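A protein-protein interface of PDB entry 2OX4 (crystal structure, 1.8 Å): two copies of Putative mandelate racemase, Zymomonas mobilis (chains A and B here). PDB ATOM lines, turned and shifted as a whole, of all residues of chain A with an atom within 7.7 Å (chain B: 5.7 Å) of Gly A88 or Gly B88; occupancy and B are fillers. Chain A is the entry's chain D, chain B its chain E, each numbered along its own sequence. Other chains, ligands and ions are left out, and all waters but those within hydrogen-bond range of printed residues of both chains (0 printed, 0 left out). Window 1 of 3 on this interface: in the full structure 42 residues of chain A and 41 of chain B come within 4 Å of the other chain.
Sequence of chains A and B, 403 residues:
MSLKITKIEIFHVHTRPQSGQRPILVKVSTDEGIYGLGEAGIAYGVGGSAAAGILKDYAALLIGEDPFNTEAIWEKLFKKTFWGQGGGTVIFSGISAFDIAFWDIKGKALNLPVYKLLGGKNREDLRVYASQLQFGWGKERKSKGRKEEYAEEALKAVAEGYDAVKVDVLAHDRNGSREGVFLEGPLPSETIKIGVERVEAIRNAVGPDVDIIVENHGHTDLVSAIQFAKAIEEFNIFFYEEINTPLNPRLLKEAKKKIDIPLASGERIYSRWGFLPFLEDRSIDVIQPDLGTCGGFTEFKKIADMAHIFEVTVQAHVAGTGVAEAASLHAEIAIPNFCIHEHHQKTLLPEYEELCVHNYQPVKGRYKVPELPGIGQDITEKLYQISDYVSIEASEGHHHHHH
O of Gly A87 sits at hydrogen-bond distance from OG1 of Thr B89. The side-chain hydroxyl (OG1) of Thr A89 sits at hydrogen-bond distance from the backbone carbonyl oxygen (O) of Gly B87, 2.9 Å away.
Of the 19 printed residues of chain A, 11 touch a printed residue of chain B. Hydrophobic or aromatic side chains of chain A that line the printed part of chain B: Trp A83, Val A90, Ile A91, Phe A92, Leu A247 and Tyr A270. Of the 11 printed residues of chain B, 9 touch a printed residue of chain A. Among the printed residues, 21 pairs touch across the chains.
The side-chain hydroxyl of Tyr A58 sits at hydrogen-bond distance from the backbone carbonyl oxygen of Ile A91 (3.1 Å). The side-chain hydroxyl (OG) of Ser A93 is in hydrogen-bond range of the backbone carbonyl oxygen (O) of Thr A89, at 2.7 Å. The side-chain hydroxyl (OG1) of Thr A89 sits at hydrogen-bond distance from the side-chain hydroxyl (OH) of Tyr A270, at 2.7 Å. The backbone carbonyl oxygen of Thr B89 lies within hydrogen-bond range of the side-chain hydroxyl of Ser B93 (2.7 Å). OG1 of Thr B89 lies within hydrogen-bond range of OH of Tyr B270, 2.7 Å away.
Among the printed residues, merely in contact across the chains: Gly A88 with Gly B88 (3.3 Å), Leu A247 with Gly B86 (3.4 Å), Gln A85 with Leu B247 (3.4 Å), Gly A86 with Leu B247 (3.5 Å), Trp A83 with Tyr B270 (3.5 Å), Trp A83 with Thr B89 (3.6 Å), Tyr A270 with Gly B86 (3.6 Å), Gly A86 with Tyr B270 (3.6 Å), Gly A86 with Thr B89 (3.9 Å), Thr A89 with Gly B86 (3.9 Å), Gly A87 with Gly B88 (3.9 Å), Val A90 with Val B90 (3.9 Å), Val A90 with Ile B91 (3.9 Å), Leu A247 with Phe B92 (3.9 Å), Phe A92 with Leu B247 (3.9 Å), Ile A91 with Val B90 (3.9 Å), Gly A88 with Gly B87 (3.9 Å), Thr A89 with Ile B91 (3.9 Å) and Ile A91 with Thr B89 (3.97 Å).
Gly A86 touches Thr B89, and with the chains exchanged Thr A89 touches Gly B86. Gly A87 touches Thr B89, and with the chains exchanged Thr A89 touches Gly B87. Val A90 touches its own counterpart, Val B90. Val A90 touches Ile B91, and with the chains exchanged Ile A91 touches Val B90.
Printed residues of chain B within 4 Å of Gly A88: Gly B87 and Gly B88. Printed residues of chain B within 4 Å of Tyr A270: Gly B86 (3.6 Å). Thr A293 touches none of the printed residues of chain B. Gly B88 touches just these residues of chain A: Gly A87 and Gly A88. Of the printed residues of chain A, Thr B89 touches Trp A83, Gly A86, Gly A87 and Ile A91. Of the printed residues of chain A, Phe B92 touches Leu A247. Of the printed residues of chain A, Leu B247 touches Gln A85, Gly A86 and Phe A92. The nearest residue of chain A that does not touch Gly B88 is Thr A89 (4.2 Å). The nearest printed residue of chain B that does not touch Val A90 is Gly B87 (5.3 Å).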
ATOM      1  N   ILE A  42      17.902 -27.600 -18.648  1.00  0.00           N
ATOM      2  CA  ILE A  42      19.266 -28.105 -18.434  1.00  0.00           C
ATOM      3  C   ILE A  42      19.516 -29.361 -19.292  1.00  0.00           C
ATOM      4  O   ILE A  42      20.172 -30.305 -18.860  1.00  0.00           O
ATOM      5  CB  ILE A  42      19.537 -28.420 -16.924  1.00  0.00           C
ATOM      6  CG1 ILE A  42      18.932 -27.346 -16.013  1.00  0.00           C
ATOM      7  CG2 ILE A  42      21.036 -28.547 -16.643  1.00  0.00           C
ATOM      8  CD1 ILE A  42      19.416 -27.415 -14.578  1.00  0.00           C
ATOM      9  N   TYR A  58      10.707 -30.856  -5.232  1.00  0.00           N
ATOM     10  CA  TYR A  58       9.650 -29.849  -5.254  1.00  0.00           C
ATOM     11  C   TYR A  58       8.280 -30.509  -5.349  1.00  0.00           C
ATOM     12  O   TYR A  58       7.311 -29.994  -4.794  1.00  0.00           O
ATOM     13  CB  TYR A  58       9.806 -28.877  -6.416  1.00  0.00           C
ATOM     14  CG  TYR A  58      10.932 -27.874  -6.291  1.00  0.00           C
ATOM     15  CD1 TYR A  58      11.231 -27.012  -7.353  1.00  0.00           C
ATOM     16  CD2 TYR A  58      11.699 -27.778  -5.123  1.00  0.00           C
ATOM     17  CE1 TYR A  58      12.285 -26.075  -7.260  1.00  0.00           C
ATOM     18  CE2 TYR A  58      12.751 -26.846  -5.023  1.00  0.00           C
ATOM     19  CZ  TYR A  58      13.031 -26.002  -6.094  1.00  0.00           C
ATOM     20  OH  TYR A  58      14.065 -25.087  -6.003  1.00  0.00           O
ATOM     21  N   TRP A  83      16.397 -23.054  -0.038  1.00  0.00           N
ATOM     22  CA  TRP A  83      17.379 -22.840  -1.110  1.00  0.00           C
ATOM     23  C   TRP A  83      16.885 -21.920  -2.212  1.00  0.00           C
ATOM     24  O   TRP A  83      17.692 -21.294  -2.900  1.00  0.00           O
ATOM     25  CB  TRP A  83      17.936 -24.192  -1.618  1.00  0.00           C
ATOM     26  CG  TRP A  83      18.403 -24.971  -0.437  1.00  0.00           C
ATOM     27  CD1 TRP A  83      17.823 -26.086   0.097  1.00  0.00           C
ATOM     28  CD2 TRP A  83      19.485 -24.621   0.440  1.00  0.00           C
ATOM     29  NE1 TRP A  83      18.490 -26.468   1.243  1.00  0.00           N
ATOM     30  CE2 TRP A  83      19.519 -25.593   1.472  1.00  0.00           C
ATOM     31  CE3 TRP A  83      20.431 -23.578   0.455  1.00  0.00           C
ATOM     32  CZ2 TRP A  83      20.465 -25.566   2.499  1.00  0.00           C
ATOM     33  CZ3 TRP A  83      21.383 -23.550   1.487  1.00  0.00           C
ATOM     34  CH2 TRP A  83      21.389 -24.544   2.490  1.00  0.00           C
ATOM     35  N   GLY A  84      15.560 -21.794  -2.335  1.00  0.00           N
ATOM     36  CA  GLY A  84      14.962 -20.776  -3.210  1.00  0.00           C
ATOM     37  C   GLY A  84      15.610 -19.396  -3.054  1.00  0.00           C
ATOM     38  O   GLY A  84      15.943 -18.737  -4.041  1.00  0.00           O
ATOM     39  N   GLN A  85      15.835 -18.973  -1.810  1.00  0.00           N
ATOM     40  CA  GLN A  85      16.355 -17.615  -1.536  1.00  0.00           C
ATOM     41  C   GLN A  85      17.849 -17.460  -1.766  1.00  0.00           C
ATOM     42  O   GLN A  85      18.372 -16.338  -1.792  1.00  0.00           O
ATOM     43  CB  GLN A  85      15.990 -17.191  -0.120  1.00  0.00           C
ATOM     44  CG  GLN A  85      14.512 -16.893   0.034  1.00  0.00           C
ATOM     45  CD  GLN A  85      14.099 -16.810   1.482  1.00  0.00           C
ATOM     46  OE1 GLN A  85      13.721 -17.818   2.085  1.00  0.00           O
ATOM     47  NE2 GLN A  85      14.154 -15.605   2.049  1.00  0.00           N
ATOM     48  N   GLY A  86      18.536 -18.583  -1.966  1.00  0.00           N
ATOM     49  CA  GLY A  86      19.943 -18.551  -2.391  1.00  0.00           C
ATOM     50  C   GLY A  86      20.081 -18.606  -3.904  1.00  0.00           C
ATOM     51  O   GLY A  86      21.099 -18.179  -4.449  1.00  0.00           O
ATOM     52  N   GLY A  87      19.041 -19.097  -4.585  1.00  0.00           N
ATOM     53  CA  GLY A  87      18.990 -19.033  -6.045  1.00  0.00           C
ATOM     54  C   GLY A  87      19.815 -20.119  -6.711  1.00  0.00           C
ATOM     55  O   GLY A  87      20.423 -20.972  -6.047  1.00  0.00           O
ATOM     56  N   GLY A  88      19.815 -20.099  -8.037  1.00  0.00           N
ATOM     57  CA  GLY A  88      20.722 -20.911  -8.814  1.00  0.00           C
ATOM     58  C   GLY A  88      20.086 -21.531 -10.043  1.00  0.00           C
ATOM     59  O   GLY A  88      18.865 -21.544 -10.176  1.00  0.00           O
ATOM     60  N   THR A  89      20.948 -22.029 -10.927  1.00  0.00           N
ATOM     61  CA  THR A  89      20.578 -22.716 -12.171  1.00  0.00           C
ATOM     62  C   THR A  89      19.525 -23.801 -11.913  1.00  0.00           C
ATOM     63  O   THR A  89      18.445 -23.788 -12.505  1.00  0.00           O
ATOM     64  CB  THR A  89      21.847 -23.391 -12.808  1.00  0.00           C
ATOM     65  OG1 THR A  89      22.861 -22.400 -13.065  1.00  0.00           O
ATOM     66  CG2 THR A  89      21.474 -24.065 -14.115  1.00  0.00           C
ATOM     67  N   VAL A  90      19.840 -24.725 -11.008  1.00  0.00           N
ATOM     68  CA  VAL A  90      19.006 -25.915 -10.800  1.00  0.00           C
ATOM     69  C   VAL A  90      17.777 -25.508  -9.984  1.00  0.00           C
ATOM     70  O   VAL A  90      16.651 -25.910 -10.308  1.00  0.00           O
ATOM     71  CB  VAL A  90      19.816 -27.031 -10.068  1.00  0.00           C
ATOM     72  CG1 VAL A  90      18.919 -28.256  -9.711  1.00  0.00           C
ATOM     73  CG2 VAL A  90      21.038 -27.457 -10.911  1.00  0.00           C
ATOM     74  N   ILE A  91      17.997 -24.700  -8.937  1.00  0.00           N
ATOM     75  CA  ILE A  91      16.914 -24.171  -8.101  1.00  0.00           C
ATOM     76  C   ILE A  91      15.817 -23.520  -8.947  1.00  0.00           C
ATOM     77  O   ILE A  91      14.649 -23.903  -8.853  1.00  0.00           O
ATOM     78  CB  ILE A  91      17.455 -23.183  -7.027  1.00  0.00           C
ATOM     79  CG1 ILE A  91      18.354 -23.918  -6.006  1.00  0.00           C
ATOM     80  CG2 ILE A  91      16.313 -22.402  -6.342  1.00  0.00           C
ATOM     81  CD1 ILE A  91      17.724 -25.117  -5.326  1.00  0.00           C
ATOM     82  N   PHE A  92      16.197 -22.586  -9.814  1.00  0.00           N
ATOM     83  CA  PHE A  92      15.224 -21.932 -10.686  1.00  0.00           C
ATOM     84  C   PHE A  92      14.659 -22.808 -11.820  1.00  0.00           C
ATOM     85  O   PHE A  92      13.496 -22.631 -12.213  1.00  0.00           O
ATOM     86  CB  PHE A  92      15.768 -20.584 -11.194  1.00  0.00           C
ATOM     87  CG  PHE A  92      15.698 -19.500 -10.161  1.00  0.00           C
ATOM     88  CD1 PHE A  92      16.851 -18.831  -9.746  1.00  0.00           C
ATOM     89  CD2 PHE A  92      14.476 -19.173  -9.571  1.00  0.00           C
ATOM     90  CE1 PHE A  92      16.783 -17.842  -8.766  1.00  0.00           C
ATOM     91  CE2 PHE A  92      14.392 -18.187  -8.584  1.00  0.00           C
ATOM     92  CZ  PHE A  92      15.540 -17.522  -8.187  1.00  0.00           C
ATOM     93  N   SER A  93      15.452 -23.760 -12.313  1.00  0.00           N
ATOM     94  CA  SER A  93      14.955 -24.715 -13.319  1.00  0.00           C
ATOM     95  C   SER A  93      13.774 -25.532 -12.804  1.00  0.00           C
ATOM     96  O   SER A  93      12.854 -25.848 -13.562  1.00  0.00           O
ATOM     97  CB  SER A  93      16.063 -25.654 -13.786  1.00  0.00           C
ATOM     98  OG  SER A  93      17.074 -24.939 -14.464  1.00  0.00           O
ATOM     99  N   GLY A  94      13.810 -25.871 -11.513  1.00  0.00           N
ATOM    100  CA  GLY A  94      12.738 -26.638 -10.886  1.00  0.00           C
ATOM    101  C   GLY A  94      11.456 -25.837 -10.850  1.00  0.00           C
ATOM    102  O   GLY A  94      10.395 -26.330 -11.237  1.00  0.00           O
ATOM    103  N   LEU A 247      28.646 -14.187 -13.821  1.00  0.00           N
ATOM    104  CA  LEU A 247      28.582 -14.202 -12.353  1.00  0.00           C
ATOM    105  C   LEU A 247      29.053 -12.929 -11.637  1.00  0.00           C
ATOM    106  O   LEU A 247      28.657 -12.693 -10.495  1.00  0.00           O
ATOM    107  CB  LEU A 247      29.338 -15.412 -11.809  1.00  0.00           C
ATOM    108  CG  LEU A 247      28.646 -16.762 -11.705  1.00  0.00           C
ATOM    109  CD1 LEU A 247      29.511 -17.679 -10.817  1.00  0.00           C
ATOM    110  CD2 LEU A 247      27.218 -16.660 -11.132  1.00  0.00           C
ATOM    111  N   TYR A 270      19.145 -15.929 -14.147  1.00  0.00           N
ATOM    112  CA  TYR A 270      17.863 -16.524 -13.719  1.00  0.00           C
ATOM    113  C   TYR A 270      17.072 -15.586 -12.816  1.00  0.00           C
ATOM    114  O   TYR A 270      17.642 -14.995 -11.896  1.00  0.00           O
ATOM    115  CB  TYR A 270      18.082 -17.863 -13.008  1.00  0.00           C
ATOM    116  CG  TYR A 270      19.215 -18.666 -13.600  1.00  0.00           C
ATOM    117  CD1 TYR A 270      19.083 -19.277 -14.846  1.00  0.00           C
ATOM    118  CD2 TYR A 270      20.431 -18.792 -12.928  1.00  0.00           C
ATOM    119  CE1 TYR A 270      20.132 -20.013 -15.404  1.00  0.00           C
ATOM    120  CE2 TYR A 270      21.491 -19.518 -13.484  1.00  0.00           C
ATOM    121  CZ  TYR A 270      21.329 -20.126 -14.716  1.00  0.00           C
ATOM    122  OH  TYR A 270      22.374 -20.853 -15.251  1.00  0.00           O
ATOM    123  N   SER A 271      15.768 -15.470 -13.084  1.00  0.00           N
ATOM    124  CA  SER A 271      14.839 -14.655 -12.284  1.00  0.00           C
ATOM    125  C   SER A 271      15.031 -13.149 -12.459  1.00  0.00           C
ATOM    126  O   SER A 271      16.064 -12.688 -12.962  1.00  0.00           O
ATOM    127  CB  SER A 271      14.879 -15.037 -10.792  1.00  0.00           C
ATOM    128  OG  SER A 271      15.909 -14.329 -10.079  1.00  0.00           O
ATOM    129  N   THR A 293      14.603 -22.137 -17.327  1.00  0.00           N
ATOM    130  CA  THR A 293      15.524 -21.837 -16.210  1.00  0.00           C
ATOM    131  C   THR A 293      15.269 -20.500 -15.508  1.00  0.00           C
ATOM    132  O   THR A 293      15.639 -20.340 -14.348  1.00  0.00           O
ATOM    133  CB  THR A 293      17.040 -21.915 -16.573  1.00  0.00           C
ATOM    134  OG1 THR A 293      17.383 -20.885 -17.513  1.00  0.00           O
ATOM    135  CG2 THR A 293      17.447 -23.304 -17.127  1.00  0.00           C
ATOM    136  N   CYS A 294      14.651 -19.541 -16.198  1.00  0.00           N
ATOM    137  CA  CYS A 294      14.486 -18.200 -15.641  1.00  0.00           C
ATOM    138  C   CYS A 294      13.404 -18.097 -14.560  1.00  0.00           C
ATOM    139  O   CYS A 294      13.349 -17.110 -13.829  1.00  0.00           O
ATOM    140  CB  CYS A 294      14.208 -17.186 -16.755  1.00  0.00           C
ATOM    141  SG  CYS A 294      12.523 -17.210 -17.365  1.00  0.00           S
ATOM    142  N   GLY B  86      26.855 -20.178 -14.615  1.00  0.00           N
ATOM    143  CA  GLY B  86      25.592 -19.586 -14.170  1.00  0.00           C
ATOM    144  C   GLY B  86      25.464 -19.569 -12.656  1.00  0.00           C
ATOM    145  O   GLY B  86      24.706 -18.759 -12.104  1.00  0.00           O
ATOM    146  N   GLY B  87      26.202 -20.464 -11.985  1.00  0.00           N
ATOM    147  CA  GLY B  87      26.221 -20.509 -10.507  1.00  0.00           C
ATOM    148  C   GLY B  87      25.011 -21.189  -9.888  1.00  0.00           C
ATOM    149  O   GLY B  87      24.126 -21.700 -10.589  1.00  0.00           O
ATOM    150  N   GLY B  88      24.967 -21.199  -8.557  1.00  0.00           N
ATOM    151  CA  GLY B  88      23.780 -21.646  -7.855  1.00  0.00           C
ATOM    152  C   GLY B  88      24.089 -22.545  -6.677  1.00  0.00           C
ATOM    153  O   GLY B  88      25.177 -23.098  -6.579  1.00  0.00           O
ATOM    154  N   THR B  89      23.109 -22.651  -5.785  1.00  0.00           N
ATOM    155  CA  THR B  89      23.154 -23.494  -4.599  1.00  0.00           C
ATOM    156  C   THR B  89      23.630 -24.905  -4.937  1.00  0.00           C
ATOM    157  O   THR B  89      24.586 -25.389  -4.344  1.00  0.00           O
ATOM    158  CB  THR B  89      21.749 -23.589  -3.965  1.00  0.00           C
ATOM    159  OG1 THR B  89      21.254 -22.273  -3.672  1.00  0.00           O
ATOM    160  CG2 THR B  89      21.797 -24.398  -2.721  1.00  0.00           C
ATOM    161  N   VAL B  90      22.966 -25.544  -5.899  1.00  0.00           N
ATOM    162  CA  VAL B  90      23.222 -26.962  -6.175  1.00  0.00           C
ATOM    163  C   VAL B  90      24.523 -27.090  -6.973  1.00  0.00           C
ATOM    164  O   VAL B  90      25.368 -27.938  -6.663  1.00  0.00           O
ATOM    165  CB  VAL B  90      22.034 -27.614  -6.944  1.00  0.00           C
ATOM    166  CG1 VAL B  90      22.328 -29.105  -7.253  1.00  0.00           C
ATOM    167  CG2 VAL B  90      20.728 -27.496  -6.135  1.00  0.00           C
ATOM    168  N   ILE B  91      24.669 -26.253  -8.010  1.00  0.00           N
ATOM    169  CA  ILE B  91      25.915 -26.194  -8.797  1.00  0.00           C
ATOM    170  C   ILE B  91      27.165 -26.123  -7.910  1.00  0.00           C
ATOM    171  O   ILE B  91      28.081 -26.937  -8.054  1.00  0.00           O
ATOM    172  CB  ILE B  91      25.882 -24.989  -9.781  1.00  0.00           C
ATOM    173  CG1 ILE B  91      24.715 -25.140 -10.777  1.00  0.00           C
ATOM    174  CG2 ILE B  91      27.244 -24.796 -10.467  1.00  0.00           C
ATOM    175  CD1 ILE B  91      24.745 -26.463 -11.574  1.00  0.00           C
ATOM    176  N   PHE B  92      27.199 -25.159  -6.986  1.00  0.00           N
ATOM    177  CA  PHE B  92      28.349 -25.005  -6.124  1.00  0.00           C
ATOM    178  C   PHE B  92      28.473 -26.076  -5.030  1.00  0.00           C
ATOM    179  O   PHE B  92      29.589 -26.393  -4.608  1.00  0.00           O
ATOM    180  CB  PHE B  92      28.436 -23.588  -5.552  1.00  0.00           C
ATOM    181  CG  PHE B  92      28.967 -22.576  -6.531  1.00  0.00           C
ATOM    182  CD1 PHE B  92      28.216 -21.454  -6.869  1.00  0.00           C
ATOM    183  CD2 PHE B  92      30.196 -22.759  -7.140  1.00  0.00           C
ATOM    184  CE1 PHE B  92      28.709 -20.516  -7.801  1.00  0.00           C
ATOM    185  CE2 PHE B  92      30.695 -21.832  -8.067  1.00  0.00           C
ATOM    186  CZ  PHE B  92      29.944 -20.712  -8.399  1.00  0.00           C
ATOM    187  N   SER B  93      27.348 -26.656  -4.601  1.00  0.00           N
ATOM    188  CA  SER B  93      27.389 -27.731  -3.610  1.00  0.00           C
ATOM    189  C   SER B  93      28.102 -28.946  -4.172  1.00  0.00           C
ATOM    190  O   SER B  93      28.785 -29.670  -3.439  1.00  0.00           O
ATOM    191  CB  SER B  93      25.984 -28.133  -3.163  1.00  0.00           C
ATOM    192  OG  SER B  93      25.369 -27.088  -2.440  1.00  0.00           O
ATOM    193  N   LEU B 247      19.496 -12.475  -2.503  1.00  0.00           N
ATOM    194  CA  LEU B 247      19.526 -12.383  -3.979  1.00  0.00           C
ATOM    195  C   LEU B 247      19.628 -10.987  -4.626  1.00  0.00           C
ATOM    196  O   LEU B 247      20.070 -10.885  -5.773  1.00  0.00           O
ATOM    197  CB  LEU B 247      18.345 -13.139  -4.586  1.00  0.00           C
ATOM    198  CG  LEU B 247      18.404 -14.646  -4.789  1.00  0.00           C
ATOM    199  CD1 LEU B 247      17.236 -15.036  -5.697  1.00  0.00           C
ATOM    200  CD2 LEU B 247      19.740 -15.108  -5.408  1.00  0.00           C
ATOM    201  N   TYR B 270      27.310 -18.031  -2.310  1.00  0.00           N
ATOM    202  CA  TYR B 270      28.223 -19.098  -2.779  1.00  0.00           C
ATOM    203  C   TYR B 270      29.349 -18.556  -3.634  1.00  0.00           C
ATOM    204  O   TYR B 270      29.106 -17.723  -4.513  1.00  0.00           O
ATOM    205  CB  TYR B 270      27.460 -20.166  -3.572  1.00  0.00           C
ATOM    206  CG  TYR B 270      26.094 -20.462  -2.999  1.00  0.00           C
ATOM    207  CD1 TYR B 270      25.961 -21.123  -1.776  1.00  0.00           C
ATOM    208  CD2 TYR B 270      24.934 -20.064  -3.670  1.00  0.00           C
ATOM    209  CE1 TYR B 270      24.700 -21.382  -1.232  1.00  0.00           C
ATOM    210  CE2 TYR B 270      23.679 -20.303  -3.136  1.00  0.00           C
ATOM    211  CZ  TYR B 270      23.562 -20.971  -1.929  1.00  0.00           C
ATOM    212  OH  TYR B 270      22.313 -21.231  -1.409  1.00  0.00           O
ATOM    213  N   THR B 293      28.759 -25.786   0.456  1.00  0.00           N
ATOM    214  CA  THR B 293      28.055 -25.038  -0.625  1.00  0.00           C
ATOM    215  C   THR B 293      28.869 -23.902  -1.237  1.00  0.00           C
ATOM    216  O   THR B 293      28.616 -23.514  -2.386  1.00  0.00           O
ATOM    217  CB  THR B 293      26.667 -24.444  -0.212  1.00  0.00           C
ATOM    218  OG1 THR B 293      26.838 -23.442   0.809  1.00  0.00           O
ATOM    219  CG2 THR B 293      25.709 -25.517   0.281  1.00  0.00           C
